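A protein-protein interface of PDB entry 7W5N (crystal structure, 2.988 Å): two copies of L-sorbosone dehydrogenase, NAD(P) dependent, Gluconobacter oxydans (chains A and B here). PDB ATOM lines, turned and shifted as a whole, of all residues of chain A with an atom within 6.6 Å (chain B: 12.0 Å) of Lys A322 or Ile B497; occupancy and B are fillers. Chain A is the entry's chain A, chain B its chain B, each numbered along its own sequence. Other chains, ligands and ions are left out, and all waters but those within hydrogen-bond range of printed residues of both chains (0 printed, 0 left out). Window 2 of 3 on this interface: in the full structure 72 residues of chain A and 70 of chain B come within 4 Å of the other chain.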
ATOM      1  N   ALA A 281     -12.428 -20.133  24.002  1.00  0.00           N
ATOM      2  CA  ALA A 281     -12.578 -20.617  25.399  1.00  0.00           C
ATOM      3  C   ALA A 281     -13.372 -21.938  25.407  1.00  0.00           C
ATOM      4  O   ALA A 281     -12.932 -22.916  26.077  1.00  0.00           O
ATOM      5  CB  ALA A 281     -13.216 -19.553  26.264  1.00  0.00           C
ATOM      6  N   ASP A 282     -14.484 -21.987  24.672  1.00  0.00           N
ATOM      7  CA  ASP A 282     -15.342 -23.197  24.555  1.00  0.00           C
ATOM      8  C   ASP A 282     -14.514 -24.349  23.960  1.00  0.00           C
ATOM      9  O   ASP A 282     -14.584 -25.488  24.498  1.00  0.00           O
ATOM     10  CB  ASP A 282     -16.611 -22.907  23.742  1.00  0.00           C
ATOM     11  CG  ASP A 282     -17.606 -24.049  23.822  1.00  0.00           C
ATOM     12  OD1 ASP A 282     -17.421 -25.040  23.053  1.00  0.00           O
ATOM     13  OD2 ASP A 282     -18.517 -23.974  24.705  1.00  0.00           O
ATOM     14  N   ALA A 285     -11.840 -25.600  26.552  1.00  0.00           N
ATOM     15  CA  ALA A 285     -12.422 -26.458  27.603  1.00  0.00           C
ATOM     16  C   ALA A 285     -12.767 -27.830  26.999  1.00  0.00           C
ATOM     17  O   ALA A 285     -12.466 -28.859  27.630  1.00  0.00           O
ATOM     18  CB  ALA A 285     -13.614 -25.780  28.223  1.00  0.00           C
ATOM     19  N   PHE A 286     -13.365 -27.861  25.805  1.00  0.00           N
ATOM     20  CA  PHE A 286     -13.708 -29.128  25.108  1.00  0.00           C
ATOM     21  C   PHE A 286     -12.422 -29.920  24.848  1.00  0.00           C
ATOM     22  O   PHE A 286     -12.384 -31.108  25.226  1.00  0.00           O
ATOM     23  CB  PHE A 286     -14.453 -28.888  23.791  1.00  0.00           C
ATOM     24  CG  PHE A 286     -14.726 -30.140  22.984  1.00  0.00           C
ATOM     25  CD1 PHE A 286     -13.816 -30.597  22.037  1.00  0.00           C
ATOM     26  CD2 PHE A 286     -15.893 -30.858  23.168  1.00  0.00           C
ATOM     27  CE1 PHE A 286     -14.076 -31.732  21.291  1.00  0.00           C
ATOM     28  CE2 PHE A 286     -16.149 -31.996  22.427  1.00  0.00           C
ATOM     29  CZ  PHE A 286     -15.246 -32.424  21.487  1.00  0.00           C
ATOM     30  N   SER A 289     -11.192 -31.366  28.144  1.00  0.00           N
ATOM     31  CA  SER A 289     -12.197 -32.034  29.006  1.00  0.00           C
ATOM     32  C   SER A 289     -12.818 -33.247  28.298  1.00  0.00           C
ATOM     33  O   SER A 289     -13.055 -34.276  28.949  1.00  0.00           O
ATOM     34  CB  SER A 289     -13.209 -31.033  29.434  1.00  0.00           C
ATOM     35  OG  SER A 289     -12.534 -29.863  29.866  1.00  0.00           O
ATOM     36  N   VAL A 317     -11.796 -21.468  32.616  1.00  0.00           N
ATOM     37  CA  VAL A 317     -12.139 -22.120  33.917  1.00  0.00           C
ATOM     38  C   VAL A 317     -13.653 -22.033  34.117  1.00  0.00           C
ATOM     39  O   VAL A 317     -14.218 -22.974  34.677  1.00  0.00           O
ATOM     40  CB  VAL A 317     -11.370 -21.585  35.143  1.00  0.00           C
ATOM     41  CG1 VAL A 317      -9.869 -21.808  35.028  1.00  0.00           C
ATOM     42  CG2 VAL A 317     -11.664 -20.134  35.431  1.00  0.00           C
ATOM     43  N   ALA A 318     -14.290 -20.977  33.631  1.00  0.00           N
ATOM     44  CA  ALA A 318     -15.748 -20.791  33.764  1.00  0.00           C
ATOM     45  C   ALA A 318     -16.472 -21.838  32.919  1.00  0.00           C
ATOM     46  O   ALA A 318     -17.488 -22.364  33.380  1.00  0.00           O
ATOM     47  CB  ALA A 318     -16.132 -19.390  33.369  1.00  0.00           C
ATOM     48  N   LYS A 319     -15.962 -22.110  31.721  1.00  0.00           N
ATOM     49  CA  LYS A 319     -16.420 -23.222  30.829  1.00  0.00           C
ATOM     50  C   LYS A 319     -16.166 -24.562  31.532  1.00  0.00           C
ATOM     51  O   LYS A 319     -17.134 -25.314  31.770  1.00  0.00           O
ATOM     52  CB  LYS A 319     -15.703 -23.170  29.472  1.00  0.00           C
ATOM     53  CG  LYS A 319     -16.182 -22.070  28.537  1.00  0.00           C
ATOM     54  CD  LYS A 319     -17.448 -22.417  27.798  1.00  0.00           C
ATOM     55  CE  LYS A 319     -17.888 -21.312  26.857  1.00  0.00           C
ATOM     56  NZ  LYS A 319     -19.166 -21.634  26.175  1.00  0.00           N
ATOM     57  N   MET A 320     -14.915 -24.824  31.906  1.00  0.00           N
ATOM     58  CA  MET A 320     -14.534 -26.076  32.601  1.00  0.00           C
ATOM     59  C   MET A 320     -15.517 -26.371  33.745  1.00  0.00           C
ATOM     60  O   MET A 320     -15.966 -27.517  33.819  1.00  0.00           O
ATOM     61  CB  MET A 320     -13.103 -25.994  33.134  1.00  0.00           C
ATOM     62  CG  MET A 320     -12.059 -26.312  32.074  1.00  0.00           C
ATOM     63  SD  MET A 320     -10.406 -26.214  32.780  1.00  0.00           S
ATOM     64  CE  MET A 320      -9.668 -27.716  32.170  1.00  0.00           C
ATOM     65  N   GLU A 321     -15.861 -25.383  34.581  1.00  0.00           N
ATOM     66  CA  GLU A 321     -16.684 -25.591  35.810  1.00  0.00           C
ATOM     67  C   GLU A 321     -18.172 -25.645  35.466  1.00  0.00           C
ATOM     68  O   GLU A 321     -18.925 -26.061  36.339  1.00  0.00           O
ATOM     69  CB  GLU A 321     -16.432 -24.518  36.873  1.00  0.00           C
ATOM     70  CG  GLU A 321     -15.484 -24.965  37.983  1.00  0.00           C
ATOM     71  CD  GLU A 321     -14.447 -23.940  38.443  1.00  0.00           C
ATOM     72  OE1 GLU A 321     -14.397 -22.820  37.879  1.00  0.00           O
ATOM     73  OE2 GLU A 321     -13.661 -24.270  39.360  1.00  0.00           O
ATOM     74  N   LYS A 322     -18.579 -25.248  34.263  1.00  0.00           N
ATOM     75  CA  LYS A 322     -19.989 -25.361  33.819  1.00  0.00           C
ATOM     76  C   LYS A 322     -20.216 -26.745  33.196  1.00  0.00           C
ATOM     77  O   LYS A 322     -21.384 -27.090  32.976  1.00  0.00           O
ATOM     78  CB  LYS A 322     -20.350 -24.242  32.840  1.00  0.00           C
ATOM     79  CG  LYS A 322     -20.664 -22.901  33.485  1.00  0.00           C
ATOM     80  CD  LYS A 322     -21.853 -22.187  32.841  1.00  0.00           C
ATOM     81  CE  LYS A 322     -21.971 -20.714  33.211  1.00  0.00           C
ATOM     82  NZ  LYS A 322     -20.905 -19.872  32.604  1.00  0.00           N
ATOM     83  N   ILE A 323     -19.157 -27.511  32.907  1.00  0.00           N
ATOM     84  CA  ILE A 323     -19.271 -28.875  32.293  1.00  0.00           C
ATOM     85  C   ILE A 323     -20.065 -29.787  33.230  1.00  0.00           C
ATOM     86  O   ILE A 323     -19.718 -29.858  34.405  1.00  0.00           O
ATOM     87  CB  ILE A 323     -17.887 -29.473  31.990  1.00  0.00           C
ATOM     88  CG1 ILE A 323     -17.299 -28.855  30.726  1.00  0.00           C
ATOM     89  CG2 ILE A 323     -17.941 -30.989  31.919  1.00  0.00           C
ATOM     90  CD1 ILE A 323     -15.830 -29.126  30.563  1.00  0.00           C
ATOM     91  N   ARG A 324     -21.062 -30.489  32.707  1.00  0.00           N
ATOM     92  CA  ARG A 324     -21.963 -31.331  33.528  1.00  0.00           C
ATOM     93  C   ARG A 324     -21.262 -32.677  33.738  1.00  0.00           C
ATOM     94  O   ARG A 324     -20.989 -33.395  32.738  1.00  0.00           O
ATOM     95  CB  ARG A 324     -23.351 -31.457  32.891  1.00  0.00           C
ATOM     96  CG  ARG A 324     -23.761 -30.287  32.003  1.00  0.00           C
ATOM     97  CD  ARG A 324     -25.192 -30.374  31.478  1.00  0.00           C
ATOM     98  NE  ARG A 324     -25.278 -30.116  30.040  1.00  0.00           N
ATOM     99  CZ  ARG A 324     -25.218 -28.909  29.469  1.00  0.00           C
ATOM    100  NH1 ARG A 324     -25.075 -27.811  30.198  1.00  0.00           N
ATOM    101  NH2 ARG A 324     -25.295 -28.795  28.157  1.00  0.00           N
ATOM    102  N   VAL A 325     -20.927 -32.977  34.995  1.00  0.00           N
ATOM    103  CA  VAL A 325     -20.278 -34.258  35.404  1.00  0.00           C
ATOM    104  C   VAL A 325     -21.339 -35.112  36.088  1.00  0.00           C
ATOM    105  O   VAL A 325     -22.015 -34.587  36.973  1.00  0.00           O
ATOM    106  CB  VAL A 325     -19.071 -34.034  36.333  1.00  0.00           C
ATOM    107  CG1 VAL A 325     -18.420 -35.351  36.721  1.00  0.00           C
ATOM    108  CG2 VAL A 325     -18.032 -33.112  35.706  1.00  0.00           C
ATOM    109  N   GLN A 334     -21.768 -34.592  30.164  1.00  0.00           N
ATOM    110  CA  GLN A 334     -20.849 -34.119  29.096  1.00  0.00           C
ATOM    111  C   GLN A 334     -19.485 -34.809  29.210  1.00  0.00           C
ATOM    112  O   GLN A 334     -18.883 -35.047  28.132  1.00  0.00           O
ATOM    113  CB  GLN A 334     -20.693 -32.601  29.162  1.00  0.00           C
ATOM    114  CG  GLN A 334     -22.031 -31.892  29.211  1.00  0.00           C
ATOM    115  CD  GLN A 334     -21.948 -30.484  28.682  1.00  0.00           C
ATOM    116  OE1 GLN A 334     -21.647 -29.541  29.410  1.00  0.00           O
ATOM    117  NE2 GLN A 334     -22.214 -30.329  27.395  1.00  0.00           N
ATOM    118  N   LYS B 492     -19.208 -19.262  12.451  1.00  0.00           N
ATOM    119  CA  LYS B 492     -19.437 -19.485  13.906  1.00  0.00           C
ATOM    120  C   LYS B 492     -19.512 -20.997  14.210  1.00  0.00           C
ATOM    121  O   LYS B 492     -20.053 -21.767  13.363  1.00  0.00           O
ATOM    122  CB  LYS B 492     -20.690 -18.738  14.377  1.00  0.00           C
ATOM    123  CG  LYS B 492     -20.587 -18.197  15.800  1.00  0.00           C
ATOM    124  CD  LYS B 492     -21.900 -18.135  16.580  1.00  0.00           C
ATOM    125  CE  LYS B 492     -21.732 -17.587  17.987  1.00  0.00           C
ATOM    126  NZ  LYS B 492     -20.611 -18.234  18.717  1.00  0.00           N
ATOM    127  N   ARG B 493     -19.070 -21.348  15.423  1.00  0.00           N
ATOM    128  CA  ARG B 493     -19.086 -22.746  15.895  1.00  0.00           C
ATOM    129  C   ARG B 493     -20.178 -22.894  16.943  1.00  0.00           C
ATOM    130  O   ARG B 493     -20.457 -21.925  17.653  1.00  0.00           O
ATOM    131  CB  ARG B 493     -17.743 -23.064  16.549  1.00  0.00           C
ATOM    132  CG  ARG B 493     -17.700 -22.827  18.053  1.00  0.00           C
ATOM    133  CD  ARG B 493     -16.349 -23.078  18.694  1.00  0.00           C
ATOM    134  NE  ARG B 493     -16.367 -24.182  19.639  1.00  0.00           N
ATOM    135  CZ  ARG B 493     -15.851 -25.382  19.404  1.00  0.00           C
ATOM    136  NH1 ARG B 493     -15.273 -25.636  18.243  1.00  0.00           N
ATOM    137  NH2 ARG B 493     -15.914 -26.324  20.326  1.00  0.00           N
ATOM    138  N   SER B 494     -20.800 -24.062  16.988  1.00  0.00           N
ATOM    139  CA  SER B 494     -21.809 -24.317  18.043  1.00  0.00           C
ATOM    140  C   SER B 494     -21.025 -24.712  19.293  1.00  0.00           C
ATOM    141  O   SER B 494     -20.268 -25.667  19.225  1.00  0.00           O
ATOM    142  CB  SER B 494     -22.865 -25.322  17.646  1.00  0.00           C
ATOM    143  OG  SER B 494     -22.301 -26.560  17.261  1.00  0.00           O
ATOM    144  N   HIS B 495     -21.136 -23.926  20.358  1.00  0.00           N
ATOM    145  CA  HIS B 495     -20.498 -24.171  21.675  1.00  0.00           C
ATOM    146  C   HIS B 495     -20.954 -25.519  22.230  1.00  0.00           C
ATOM    147  O   HIS B 495     -22.125 -25.894  22.059  1.00  0.00           O
ATOM    148  CB  HIS B 495     -20.791 -23.009  22.632  1.00  0.00           C
ATOM    149  CG  HIS B 495     -20.076 -21.758  22.243  1.00  0.00           C
ATOM    150  ND1 HIS B 495     -19.856 -20.723  23.136  1.00  0.00           N
ATOM    151  CD2 HIS B 495     -19.503 -21.390  21.072  1.00  0.00           C
ATOM    152  CE1 HIS B 495     -19.182 -19.768  22.529  1.00  0.00           C
ATOM    153  NE2 HIS B 495     -18.963 -20.152  21.255  1.00  0.00           N
ATOM    154  N   TRP B 496     -20.013 -26.231  22.841  1.00  0.00           N
ATOM    155  CA  TRP B 496     -20.211 -27.524  23.534  1.00  0.00           C
ATOM    156  C   TRP B 496     -20.870 -27.262  24.876  1.00  0.00           C
ATOM    157  O   TRP B 496     -21.701 -28.083  25.287  1.00  0.00           O
ATOM    158  CB  TRP B 496     -18.863 -28.220  23.723  1.00  0.00           C
ATOM    159  CG  TRP B 496     -18.937 -29.531  24.442  1.00  0.00           C
ATOM    160  CD1 TRP B 496     -19.765 -30.586  24.166  1.00  0.00           C
ATOM    161  CD2 TRP B 496     -18.110 -29.942  25.547  1.00  0.00           C
ATOM    162  NE1 TRP B 496     -19.521 -31.619  25.033  1.00  0.00           N
ATOM    163  CE2 TRP B 496     -18.498 -31.260  25.880  1.00  0.00           C
ATOM    164  CE3 TRP B 496     -17.077 -29.334  26.272  1.00  0.00           C
ATOM    165  CZ2 TRP B 496     -17.876 -31.971  26.911  1.00  0.00           C
ATOM    166  CZ3 TRP B 496     -16.468 -30.036  27.288  1.00  0.00           C
ATOM    167  CH2 TRP B 496     -16.861 -31.339  27.599  1.00  0.00           C
ATOM    168  N   ILE B 497     -20.479 -26.172  25.536  1.00  0.00           N
ATOM    169  CA  ILE B 497     -20.882 -25.920  26.944  1.00  0.00           C
ATOM    170  C   ILE B 497     -22.005 -24.879  26.965  1.00  0.00           C
ATOM    171  O   ILE B 497     -21.838 -23.799  26.356  1.00  0.00           O
ATOM    172  CB  ILE B 497     -19.656 -25.568  27.812  1.00  0.00           C
ATOM    173  CG1 ILE B 497     -18.881 -26.844  28.169  1.00  0.00           C
ATOM    174  CG2 ILE B 497     -20.057 -24.795  29.063  1.00  0.00           C
ATOM    175  CD1 ILE B 497     -17.370 -26.705  28.121  1.00  0.00           C
ATOM    176  N   SER B 498     -23.127 -25.282  27.576  1.00  0.00           N
ATOM    177  CA  SER B 498     -24.310 -24.463  27.958  1.00  0.00           C
ATOM    178  C   SER B 498     -24.725 -23.530  26.813  1.00  0.00           C
ATOM    179  O   SER B 498     -25.244 -22.464  27.115  1.00  0.00           O
ATOM    180  CB  SER B 498     -24.060 -23.713  29.277  1.00  0.00           C
ATOM    181  OG  SER B 498     -23.351 -22.488  29.087  1.00  0.00           O
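The side-chain carboxylate (OD1) of Asp A282 lies within salt-bridge range of the guanidinium group (NH2) of Arg B493.
OD1 of Asp A282 lies within hydrogen-bond range of N of Trp B496 (2.9 Å).
The side-chain carboxylate (OD2) of Asp A282 sits at hydrogen-bond distance from the backbone NH (N) of Ile B497, at 3.1 Å.
ND1 of His B495 lies within hydrogen-bond range of NZ of Lys A319 (3.2 Å).
NZ of Lys A319 is in hydrogen-bond range of O of Ile B497, at 3.4 Å.
NE2 of Gln A334 lies within hydrogen-bond range of O of Trp B496 (3.1 Å).
OD2 of Asp A282 lies within salt-bridge range of NZ of Lys A319 (2.8 Å).
The backbone carbonyl oxygen (O) of Ala A285 lies within hydrogen-bond range of the side-chain hydroxyl (OG) of Ser A289 (2.5 Å).
The backbone NH of Gln A334 sits at hydrogen-bond distance from the backbone carbonyl oxygen of Arg A324 (2.9 Å).
His B495 touches Asp A282.
CD1 of Ile B497 touches CB of Ala A285, at 3.9 Å.
Phe A286 touches Trp B496.
Lys A322 touches Ile B497 (CB to CG2, 3.8 Å).
Ile A323 touches Trp B496.
Ile A323 touches Ile B497.
Lys A322 touches just one residue of chain B: Ile B497.
Of the printed residues of chain A, Ile B497 touches Asp A282 (3.1 Å), Ala A285 (3.9 Å), Lys A319 (3.4 Å), Lys A322 (3.8 Å) and Ile A323 (3.4 Å).
Of chain B, only Arg B493, His B495, Trp B496 and Ile B497 come within 4 Å of Asp A282.
Of chain B, only Ile B497 (3.9 Å) comes within 4 Å of Ala A285.
Lys A319 touches two residues of chain B.
No residue of chain B comes within 4 Å of Glu A321.
Ile A323 touches just these residues of chain B: Trp B496 and Ile B497.
No residue of chain B comes within 4 Å of Arg A324.
Of the printed residues of chain B, Phe A286 touches Trp B496 (3.4 Å).
Of the printed residues of chain A, Arg B493 touches Asp A282.
Printed residues of chain A within 4 Å of His B495: Asp A282 (3.2 Å) and Lys A319 (3.2 Å).
Of the printed residues of chain A, Trp B496 touches Asp A282, Phe A286, Ile A323 and Gln A334.
Printed residues of chain B within 4 Å of Gln A334: Trp B496.
Ser B498 touches none of the printed residues of chain A.
Lys B492 touches none of the printed residues of chain A.
The nearest residue of chain A that does not touch Ile B497 is Gln A334 (4.1 Å).
The nearest printed residue of chain B that does not touch Gln A334 is Ile B497 (4.1 Å).
Hydrophobic or aromatic side chains of chain B within 4 Å of the printed part of chain A: His B495, Trp B496 and Ile B497.
Hydrophobic or aromatic side chains of chain A within 4 Å of the printed part of chain B: Ala A285, Phe A286 and Ile A323.
Among the printed residues, 12 pairs touch across the chains.
No position is printed for both chains.
Of the 12 pairs that touch across the chains among the printed residues, none has its exchanged pair printed and touching as well.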
